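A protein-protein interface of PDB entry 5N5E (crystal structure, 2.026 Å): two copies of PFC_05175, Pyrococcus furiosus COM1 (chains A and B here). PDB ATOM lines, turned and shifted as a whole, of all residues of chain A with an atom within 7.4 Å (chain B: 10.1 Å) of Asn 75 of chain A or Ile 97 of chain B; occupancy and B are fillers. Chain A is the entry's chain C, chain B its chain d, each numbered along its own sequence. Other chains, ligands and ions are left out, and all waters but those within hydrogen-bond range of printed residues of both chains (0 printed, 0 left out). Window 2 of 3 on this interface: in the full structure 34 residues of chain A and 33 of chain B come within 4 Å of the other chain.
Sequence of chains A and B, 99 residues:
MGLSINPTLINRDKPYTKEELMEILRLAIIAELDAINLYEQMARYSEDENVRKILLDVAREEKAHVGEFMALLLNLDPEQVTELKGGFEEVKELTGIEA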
ATOM      1  N   LEU A  25     -22.917  11.537 -21.369  1.00  0.00           N
ATOM      2  CA  LEU A  25     -22.186  11.757 -20.126  1.00  0.00           C
ATOM      3  C   LEU A  25     -21.818  13.226 -19.960  1.00  0.00           C
ATOM      4  O   LEU A  25     -21.914  13.772 -18.856  1.00  0.00           O
ATOM      5  CB  LEU A  25     -20.937  10.875 -20.079  1.00  0.00           C
ATOM      6  CG  LEU A  25     -21.171   9.378 -19.841  1.00  0.00           C
ATOM      7  CD1 LEU A  25     -19.876   8.601 -20.003  1.00  0.00           C
ATOM      8  CD2 LEU A  25     -21.763   9.129 -18.459  1.00  0.00           C
ATOM      9  N   PHE A  69     -20.190  10.931 -13.031  1.00  0.00           N
ATOM     10  CA  PHE A  69     -20.267  11.035 -14.482  1.00  0.00           C
ATOM     11  C   PHE A  69     -18.902  11.334 -15.088  1.00  0.00           C
ATOM     12  O   PHE A  69     -18.568  10.816 -16.158  1.00  0.00           O
ATOM     13  CB  PHE A  69     -21.280  12.107 -14.879  1.00  0.00           C
ATOM     14  CG  PHE A  69     -22.703  11.750 -14.548  1.00  0.00           C
ATOM     15  CD1 PHE A  69     -23.222  10.512 -14.894  1.00  0.00           C
ATOM     16  CD2 PHE A  69     -23.522  12.653 -13.893  1.00  0.00           C
ATOM     17  CE1 PHE A  69     -24.531  10.184 -14.592  1.00  0.00           C
ATOM     18  CE2 PHE A  69     -24.832  12.330 -13.588  1.00  0.00           C
ATOM     19  CZ  PHE A  69     -25.337  11.093 -13.938  1.00  0.00           C
ATOM     20  N   MET A  70     -18.099  12.166 -14.419  1.00  0.00           N
ATOM     21  CA  MET A  70     -16.755  12.450 -14.914  1.00  0.00           C
ATOM     22  C   MET A  70     -15.903  11.186 -14.938  1.00  0.00           C
ATOM     23  O   MET A  70     -15.130  10.968 -15.880  1.00  0.00           O
ATOM     24  CB  MET A  70     -16.097  13.526 -14.052  1.00  0.00           C
ATOM     25  CG  MET A  70     -14.643  13.809 -14.400  1.00  0.00           C
ATOM     26  SD  MET A  70     -14.331  15.558 -14.688  1.00  0.00           S
ATOM     27  CE  MET A  70     -15.278  15.809 -16.184  1.00  0.00           C
ATOM     28  N   ALA A  71     -16.025  10.343 -13.912  1.00  0.00           N
ATOM     29  CA  ALA A  71     -15.270   9.095 -13.894  1.00  0.00           C
ATOM     30  C   ALA A  71     -15.603   8.238 -15.107  1.00  0.00           C
ATOM     31  O   ALA A  71     -14.705   7.686 -15.754  1.00  0.00           O
ATOM     32  CB  ALA A  71     -15.556   8.329 -12.602  1.00  0.00           C
ATOM     33  N   LEU A  72     -16.891   8.125 -15.439  1.00  0.00           N
ATOM     34  CA  LEU A  72     -17.288   7.358 -16.615  1.00  0.00           C
ATOM     35  C   LEU A  72     -16.763   7.997 -17.893  1.00  0.00           C
ATOM     36  O   LEU A  72     -16.299   7.296 -18.799  1.00  0.00           O
ATOM     37  CB  LEU A  72     -18.811   7.240 -16.672  1.00  0.00           C
ATOM     38  CG  LEU A  72     -19.483   6.483 -15.528  1.00  0.00           C
ATOM     39  CD1 LEU A  72     -20.990   6.636 -15.628  1.00  0.00           C
ATOM     40  CD2 LEU A  72     -19.093   5.014 -15.541  1.00  0.00           C
ATOM     41  N   LEU A  73     -16.854   9.325 -17.995  1.00  0.00           N
ATOM     42  CA  LEU A  73     -16.401  10.012 -19.200  1.00  0.00           C
ATOM     43  C   LEU A  73     -14.903   9.830 -19.405  1.00  0.00           C
ATOM     44  O   LEU A  73     -14.450   9.513 -20.511  1.00  0.00           O
ATOM     45  CB  LEU A  73     -16.757  11.497 -19.122  1.00  0.00           C
ATOM     46  CG  LEU A  73     -16.252  12.374 -20.271  1.00  0.00           C
ATOM     47  CD1 LEU A  73     -16.843  11.927 -21.594  1.00  0.00           C
ATOM     48  CD2 LEU A  73     -16.575  13.837 -20.004  1.00  0.00           C
ATOM     49  N   LEU A  74     -14.114  10.041 -18.349  1.00  0.00           N
ATOM     50  CA  LEU A  74     -12.669   9.878 -18.461  1.00  0.00           C
ATOM     51  C   LEU A  74     -12.307   8.459 -18.877  1.00  0.00           C
ATOM     52  O   LEU A  74     -11.345   8.247 -19.624  1.00  0.00           O
ATOM     53  CB  LEU A  74     -12.004  10.236 -17.132  1.00  0.00           C
ATOM     54  CG  LEU A  74     -12.121  11.701 -16.703  1.00  0.00           C
ATOM     55  CD1 LEU A  74     -11.622  11.888 -15.279  1.00  0.00           C
ATOM     56  CD2 LEU A  74     -11.351  12.605 -17.653  1.00  0.00           C
ATOM     57  N   ASN A  75     -13.074   7.472 -18.407  1.00  0.00           N
ATOM     58  CA  ASN A  75     -12.814   6.087 -18.782  1.00  0.00           C
ATOM     59  C   ASN A  75     -13.138   5.828 -20.250  1.00  0.00           C
ATOM     60  O   ASN A  75     -12.485   4.996 -20.887  1.00  0.00           O
ATOM     61  CB  ASN A  75     -13.619   5.149 -17.885  1.00  0.00           C
ATOM     62  CG  ASN A  75     -13.365   3.688 -18.192  1.00  0.00           C
ATOM     63  OD1 ASN A  75     -12.336   3.133 -17.807  1.00  0.00           O
ATOM     64  ND2 ASN A  75     -14.308   3.053 -18.879  1.00  0.00           N
ATOM     65  N   LEU A  76     -14.129   6.529 -20.803  1.00  0.00           N
ATOM     66  CA  LEU A  76     -14.536   6.331 -22.189  1.00  0.00           C
ATOM     67  C   LEU A  76     -13.918   7.332 -23.157  1.00  0.00           C
ATOM     68  O   LEU A  76     -13.987   7.113 -24.370  1.00  0.00           O
ATOM     69  CB  LEU A  76     -16.065   6.401 -22.304  1.00  0.00           C
ATOM     70  CG  LEU A  76     -16.847   5.314 -21.562  1.00  0.00           C
ATOM     71  CD1 LEU A  76     -18.339   5.598 -21.635  1.00  0.00           C
ATOM     72  CD2 LEU A  76     -16.537   3.930 -22.119  1.00  0.00           C
ATOM     73  N   ASP A  77     -13.314   8.414 -22.658  1.00  0.00           N
ATOM     74  CA  ASP A  77     -12.764   9.486 -23.486  1.00  0.00           C
ATOM     75  C   ASP A  77     -11.296   9.676 -23.116  1.00  0.00           C
ATOM     76  O   ASP A  77     -10.947  10.614 -22.384  1.00  0.00           O
ATOM     77  CB  ASP A  77     -13.550  10.784 -23.302  1.00  0.00           C
ATOM     78  CG  ASP A  77     -13.174  11.846 -24.320  1.00  0.00           C
ATOM     79  OD1 ASP A  77     -12.151  11.671 -25.017  1.00  0.00           O
ATOM     80  OD2 ASP A  77     -13.901  12.859 -24.422  1.00  0.00           O
ATOM     81  N   PRO A  78     -10.404   8.817 -23.620  1.00  0.00           N
ATOM     82  CA  PRO A  78      -8.981   8.954 -23.263  1.00  0.00           C
ATOM     83  C   PRO A  78      -8.382  10.298 -23.631  1.00  0.00           C
ATOM     84  O   PRO A  78      -7.475  10.774 -22.936  1.00  0.00           O
ATOM     85  CB  PRO A  78      -8.311   7.812 -24.042  1.00  0.00           C
ATOM     86  CG  PRO A  78      -9.273   7.461 -25.131  1.00  0.00           C
ATOM     87  CD  PRO A  78     -10.634   7.715 -24.569  1.00  0.00           C
ATOM     88  N   GLN A  80      -9.805  13.132 -23.277  1.00  0.00           N
ATOM     89  CA  GLN A  80     -10.135  14.038 -22.180  1.00  0.00           C
ATOM     90  C   GLN A  80      -9.188  13.864 -20.997  1.00  0.00           C
ATOM     91  O   GLN A  80      -8.858  14.846 -20.325  1.00  0.00           O
ATOM     92  CB  GLN A  80     -11.583  13.815 -21.737  1.00  0.00           C
ATOM     93  CG  GLN A  80     -12.065  14.761 -20.641  1.00  0.00           C
ATOM     94  CD  GLN A  80     -12.045  16.215 -21.072  1.00  0.00           C
ATOM     95  OE1 GLN A  80     -12.953  16.683 -21.760  1.00  0.00           O
ATOM     96  NE2 GLN A  80     -11.009  16.941 -20.665  1.00  0.00           N
ATOM     97  N   VAL A  81      -8.733  12.638 -20.732  1.00  0.00           N
ATOM     98  CA  VAL A  81      -7.781  12.421 -19.644  1.00  0.00           C
ATOM     99  C   VAL A  81      -6.507  13.217 -19.899  1.00  0.00           C
ATOM    100  O   VAL A  81      -6.034  13.962 -19.032  1.00  0.00           O
ATOM    101  CB  VAL A  81      -7.483  10.919 -19.481  1.00  0.00           C
ATOM    102  CG1 VAL A  81      -6.450  10.690 -18.382  1.00  0.00           C
ATOM    103  CG2 VAL A  81      -8.760  10.152 -19.187  1.00  0.00           C
ATOM    104  N   LYS B  85     -13.719  13.259  -5.515  1.00  0.00           N
ATOM    105  CA  LYS B  85     -13.093  12.015  -5.083  1.00  0.00           C
ATOM    106  C   LYS B  85     -14.135  11.025  -4.577  1.00  0.00           C
ATOM    107  O   LYS B  85     -14.050   9.825  -4.864  1.00  0.00           O
ATOM    108  CB  LYS B  85     -12.049  12.301  -4.004  1.00  0.00           C
ATOM    109  CG  LYS B  85     -11.323  11.062  -3.509  1.00  0.00           C
ATOM    110  CD  LYS B  85     -10.082  11.426  -2.709  1.00  0.00           C
ATOM    111  CE  LYS B  85      -9.387  10.189  -2.161  1.00  0.00           C
ATOM    112  NZ  LYS B  85     -10.226   9.474  -1.158  1.00  0.00           N
ATOM    113  N   GLY B  86     -15.127  11.505  -3.826  1.00  0.00           N
ATOM    114  CA  GLY B  86     -16.203  10.625  -3.402  1.00  0.00           C
ATOM    115  C   GLY B  86     -16.966  10.042  -4.577  1.00  0.00           C
ATOM    116  O   GLY B  86     -17.343   8.868  -4.565  1.00  0.00           O
ATOM    117  N   GLY B  87     -17.193  10.851  -5.613  1.00  0.00           N
ATOM    118  CA  GLY B  87     -17.861  10.344  -6.799  1.00  0.00           C
ATOM    119  C   GLY B  87     -17.035   9.301  -7.527  1.00  0.00           C
ATOM    120  O   GLY B  87     -17.567   8.283  -7.984  1.00  0.00           O
ATOM    121  N   PHE B  88     -15.729   9.539  -7.656  1.00  0.00           N
ATOM    122  CA  PHE B  88     -14.851   8.536  -8.251  1.00  0.00           C
ATOM    123  C   PHE B  88     -14.922   7.220  -7.485  1.00  0.00           C
ATOM    124  O   PHE B  88     -15.016   6.145  -8.089  1.00  0.00           O
ATOM    125  CB  PHE B  88     -13.407   9.048  -8.287  1.00  0.00           C
ATOM    126  CG  PHE B  88     -13.140  10.085  -9.353  1.00  0.00           C
ATOM    127  CD1 PHE B  88     -14.172  10.654 -10.082  1.00  0.00           C
ATOM    128  CD2 PHE B  88     -11.840  10.479  -9.628  1.00  0.00           C
ATOM    129  CE1 PHE B  88     -13.911  11.600 -11.060  1.00  0.00           C
ATOM    130  CE2 PHE B  88     -11.575  11.425 -10.604  1.00  0.00           C
ATOM    131  CZ  PHE B  88     -12.612  11.985 -11.320  1.00  0.00           C
ATOM    132  N   GLU B  89     -14.890   7.284  -6.151  1.00  0.00           N
ATOM    133  CA  GLU B  89     -14.922   6.068  -5.344  1.00  0.00           C
ATOM    134  C   GLU B  89     -16.248   5.332  -5.495  1.00  0.00           C
ATOM    135  O   GLU B  89     -16.277   4.095  -5.518  1.00  0.00           O
ATOM    136  CB  GLU B  89     -14.661   6.406  -3.876  1.00  0.00           C
ATOM    137  CG  GLU B  89     -13.232   6.842  -3.593  1.00  0.00           C
ATOM    138  CD  GLU B  89     -13.036   7.336  -2.170  1.00  0.00           C
ATOM    139  OE1 GLU B  89     -14.040   7.447  -1.432  1.00  0.00           O
ATOM    140  OE2 GLU B  89     -11.879   7.617  -1.792  1.00  0.00           O
ATOM    141  N   GLU B  90     -17.359   6.068  -5.581  1.00  0.00           N
ATOM    142  CA  GLU B  90     -18.656   5.419  -5.749  1.00  0.00           C
ATOM    143  C   GLU B  90     -18.718   4.634  -7.054  1.00  0.00           C
ATOM    144  O   GLU B  90     -19.222   3.507  -7.084  1.00  0.00           O
ATOM    145  CB  GLU B  90     -19.776   6.460  -5.693  1.00  0.00           C
ATOM    146  CG  GLU B  90     -21.178   5.869  -5.785  1.00  0.00           C
ATOM    147  CD  GLU B  90     -21.534   5.015  -4.583  1.00  0.00           C
ATOM    148  OE1 GLU B  90     -21.229   5.430  -3.445  1.00  0.00           O
ATOM    149  OE2 GLU B  90     -22.110   3.924  -4.776  1.00  0.00           O
ATOM    150  N   VAL B  91     -18.204   5.208  -8.144  1.00  0.00           N
ATOM    151  CA  VAL B  91     -18.188   4.488  -9.413  1.00  0.00           C
ATOM    152  C   VAL B  91     -17.319   3.242  -9.296  1.00  0.00           C
ATOM    153  O   VAL B  91     -17.695   2.158  -9.757  1.00  0.00           O
ATOM    154  CB  VAL B  91     -17.711   5.415 -10.548  1.00  0.00           C
ATOM    155  CG1 VAL B  91     -17.409   4.621 -11.815  1.00  0.00           C
ATOM    156  CG2 VAL B  91     -18.754   6.489 -10.830  1.00  0.00           C
ATOM    157  N   LYS B  92     -16.145   3.380  -8.677  1.00  0.00           N
ATOM    158  CA  LYS B  92     -15.279   2.228  -8.443  1.00  0.00           C
ATOM    159  C   LYS B  92     -16.020   1.128  -7.694  1.00  0.00           C
ATOM    160  O   LYS B  92     -15.919  -0.053  -8.046  1.00  0.00           O
ATOM    161  CB  LYS B  92     -14.039   2.668  -7.660  1.00  0.00           C
ATOM    162  CG  LYS B  92     -13.067   1.550  -7.295  1.00  0.00           C
ATOM    163  CD  LYS B  92     -12.337   1.871  -5.998  1.00  0.00           C
ATOM    164  CE  LYS B  92     -11.444   0.725  -5.554  1.00  0.00           C
ATOM    165  NZ  LYS B  92     -10.280   0.536  -6.461  1.00  0.00           N
ATOM    166  N   GLU B  93     -16.774   1.498  -6.656  1.00  0.00           N
ATOM    167  CA  GLU B  93     -17.470   0.500  -5.852  1.00  0.00           C
ATOM    168  C   GLU B  93     -18.574  -0.182  -6.650  1.00  0.00           C
ATOM    169  O   GLU B  93     -18.823  -1.381  -6.474  1.00  0.00           O
ATOM    170  CB  GLU B  93     -18.048   1.153  -4.596  1.00  0.00           C
ATOM    171  CG  GLU B  93     -18.787   0.189  -3.677  1.00  0.00           C
ATOM    172  CD  GLU B  93     -19.425   0.885  -2.493  1.00  0.00           C
ATOM    173  OE1 GLU B  93     -19.495   2.132  -2.499  1.00  0.00           O
ATOM    174  OE2 GLU B  93     -19.859   0.185  -1.555  1.00  0.00           O
ATOM    175  N   LEU B  94     -19.246   0.560  -7.529  1.00  0.00           N
ATOM    176  CA  LEU B  94     -20.417   0.037  -8.219  1.00  0.00           C
ATOM    177  C   LEU B  94     -20.076  -0.677  -9.519  1.00  0.00           C
ATOM    178  O   LEU B  94     -20.829  -1.560  -9.944  1.00  0.00           O
ATOM    179  CB  LEU B  94     -21.399   1.175  -8.509  1.00  0.00           C
ATOM    180  CG  LEU B  94     -22.048   1.837  -7.290  1.00  0.00           C
ATOM    181  CD1 LEU B  94     -22.859   3.052  -7.711  1.00  0.00           C
ATOM    182  CD2 LEU B  94     -22.924   0.851  -6.530  1.00  0.00           C
ATOM    183  N   THR B  95     -18.959  -0.325 -10.154  1.00  0.00           N
ATOM    184  CA  THR B  95     -18.609  -0.867 -11.461  1.00  0.00           C
ATOM    185  C   THR B  95     -17.180  -1.370 -11.569  1.00  0.00           C
ATOM    186  O   THR B  95     -16.875  -2.084 -12.532  1.00  0.00           O
ATOM    187  CB  THR B  95     -18.827   0.188 -12.559  1.00  0.00           C
ATOM    188  OG1 THR B  95     -17.852   1.229 -12.421  1.00  0.00           O
ATOM    189  CG2 THR B  95     -20.230   0.781 -12.474  1.00  0.00           C
ATOM    190  N   GLY B  96     -16.292  -1.021 -10.639  1.00  0.00           N
ATOM    191  CA  GLY B  96     -14.890  -1.350 -10.765  1.00  0.00           C
ATOM    192  C   GLY B  96     -14.089  -0.404 -11.631  1.00  0.00           C
ATOM    193  O   GLY B  96     -12.859  -0.532 -11.683  1.00  0.00           O
ATOM    194  N   ILE B  97     -14.737   0.546 -12.308  1.00  0.00           N
ATOM    195  CA  ILE B  97     -14.014   1.508 -13.129  1.00  0.00           C
ATOM    196  C   ILE B  97     -13.230   2.450 -12.228  1.00  0.00           C
ATOM    197  O   ILE B  97     -13.728   2.912 -11.192  1.00  0.00           O
ATOM    198  CB  ILE B  97     -14.989   2.280 -14.037  1.00  0.00           C
ATOM    199  CG1 ILE B  97     -15.619   1.334 -15.061  1.00  0.00           C
ATOM    200  CG2 ILE B  97     -14.280   3.439 -14.737  1.00  0.00           C
ATOM    201  CD1 ILE B  97     -16.790   1.928 -15.812  1.00  0.00           C
ATOM    202  N   GLU B  98     -11.994   2.740 -12.621  1.00  0.00           N
ATOM    203  CA  GLU B  98     -11.121   3.605 -11.840  1.00  0.00           C
ATOM    204  C   GLU B  98     -10.416   4.615 -12.741  1.00  0.00           C
ATOM    205  O   GLU B  98      -9.500   4.263 -13.483  1.00  0.00           O
ATOM    206  CB  GLU B  98     -10.094   2.771 -11.076  1.00  0.00           C
ATOM    207  CG  GLU B  98      -9.229   3.574 -10.118  1.00  0.00           C
ATOM    208  CD  GLU B  98      -8.302   2.696  -9.300  1.00  0.00           C
ATOM    209  OE1 GLU B  98      -8.258   1.474  -9.558  1.00  0.00           O
ATOM    210  OE2 GLU B  98      -7.621   3.227  -8.397  1.00  0.00           O
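Among the printed residues, pairs that only touch across the chains: Ala 71 of chain A with Phe 88 of chain B (3.7 Å), Leu 72 of chain A with Ile 97 of chain B (3.9 Å) and Asn 75 of chain A with Ile 97 of chain B (3.6 Å).
Printed residues of chain B that touch a printed residue of chain A: Phe 88 and Ile 97. Hydrophobic or aromatic side chains of chain B within 4 Å of the printed part of chain A: Phe 88 and Ile 97. Printed residues of chain A that touch a printed residue of chain B: Ala 71, Leu 72 and Asn 75. Hydrophobic or aromatic side chains of chain A within 4 Å of the printed part of chain B: Ala 71 and Leu 72. Among the printed residues, 3 pairs touch across the chains. Among the printed residues, no Asp or Glu carboxylate lies within 4 Å of a Lys or Arg side-chain nitrogen of the other chain.
The side-chain hydroxyl of Thr 95 of chain B lies within hydrogen-bond range of the backbone NH of Ile 97 of chain B (3.2 Å).
No position is printed for both chains. Of the 3 pairs that touch across the chains among the printed residues, none has its exchanged pair printed and touching as well.
Ile 97 of chain B touches just these residues of chain A: Leu 72 and Asn 75. No residue of chain B comes within 4 Å of Leu 74 of chain A. No residue of chain B comes within 4 Å of Leu 76 of chain A. Of the printed residues of chain A, Phe 88 of chain B touches Ala 71 (3.7 Å). Printed residues of chain B within 4 Å of Ala 71 of chain A: Phe 88. Glu 98 of chain B touches none of the printed residues of chain A. The nearest residue of chain B that does not touch Asn 75 of chain A is Glu 98 of chain B (5.2 Å). The nearest printed residue of chain B that does not touch Ala 71 of chain A is Val 91 of chain B (4.1 Å).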
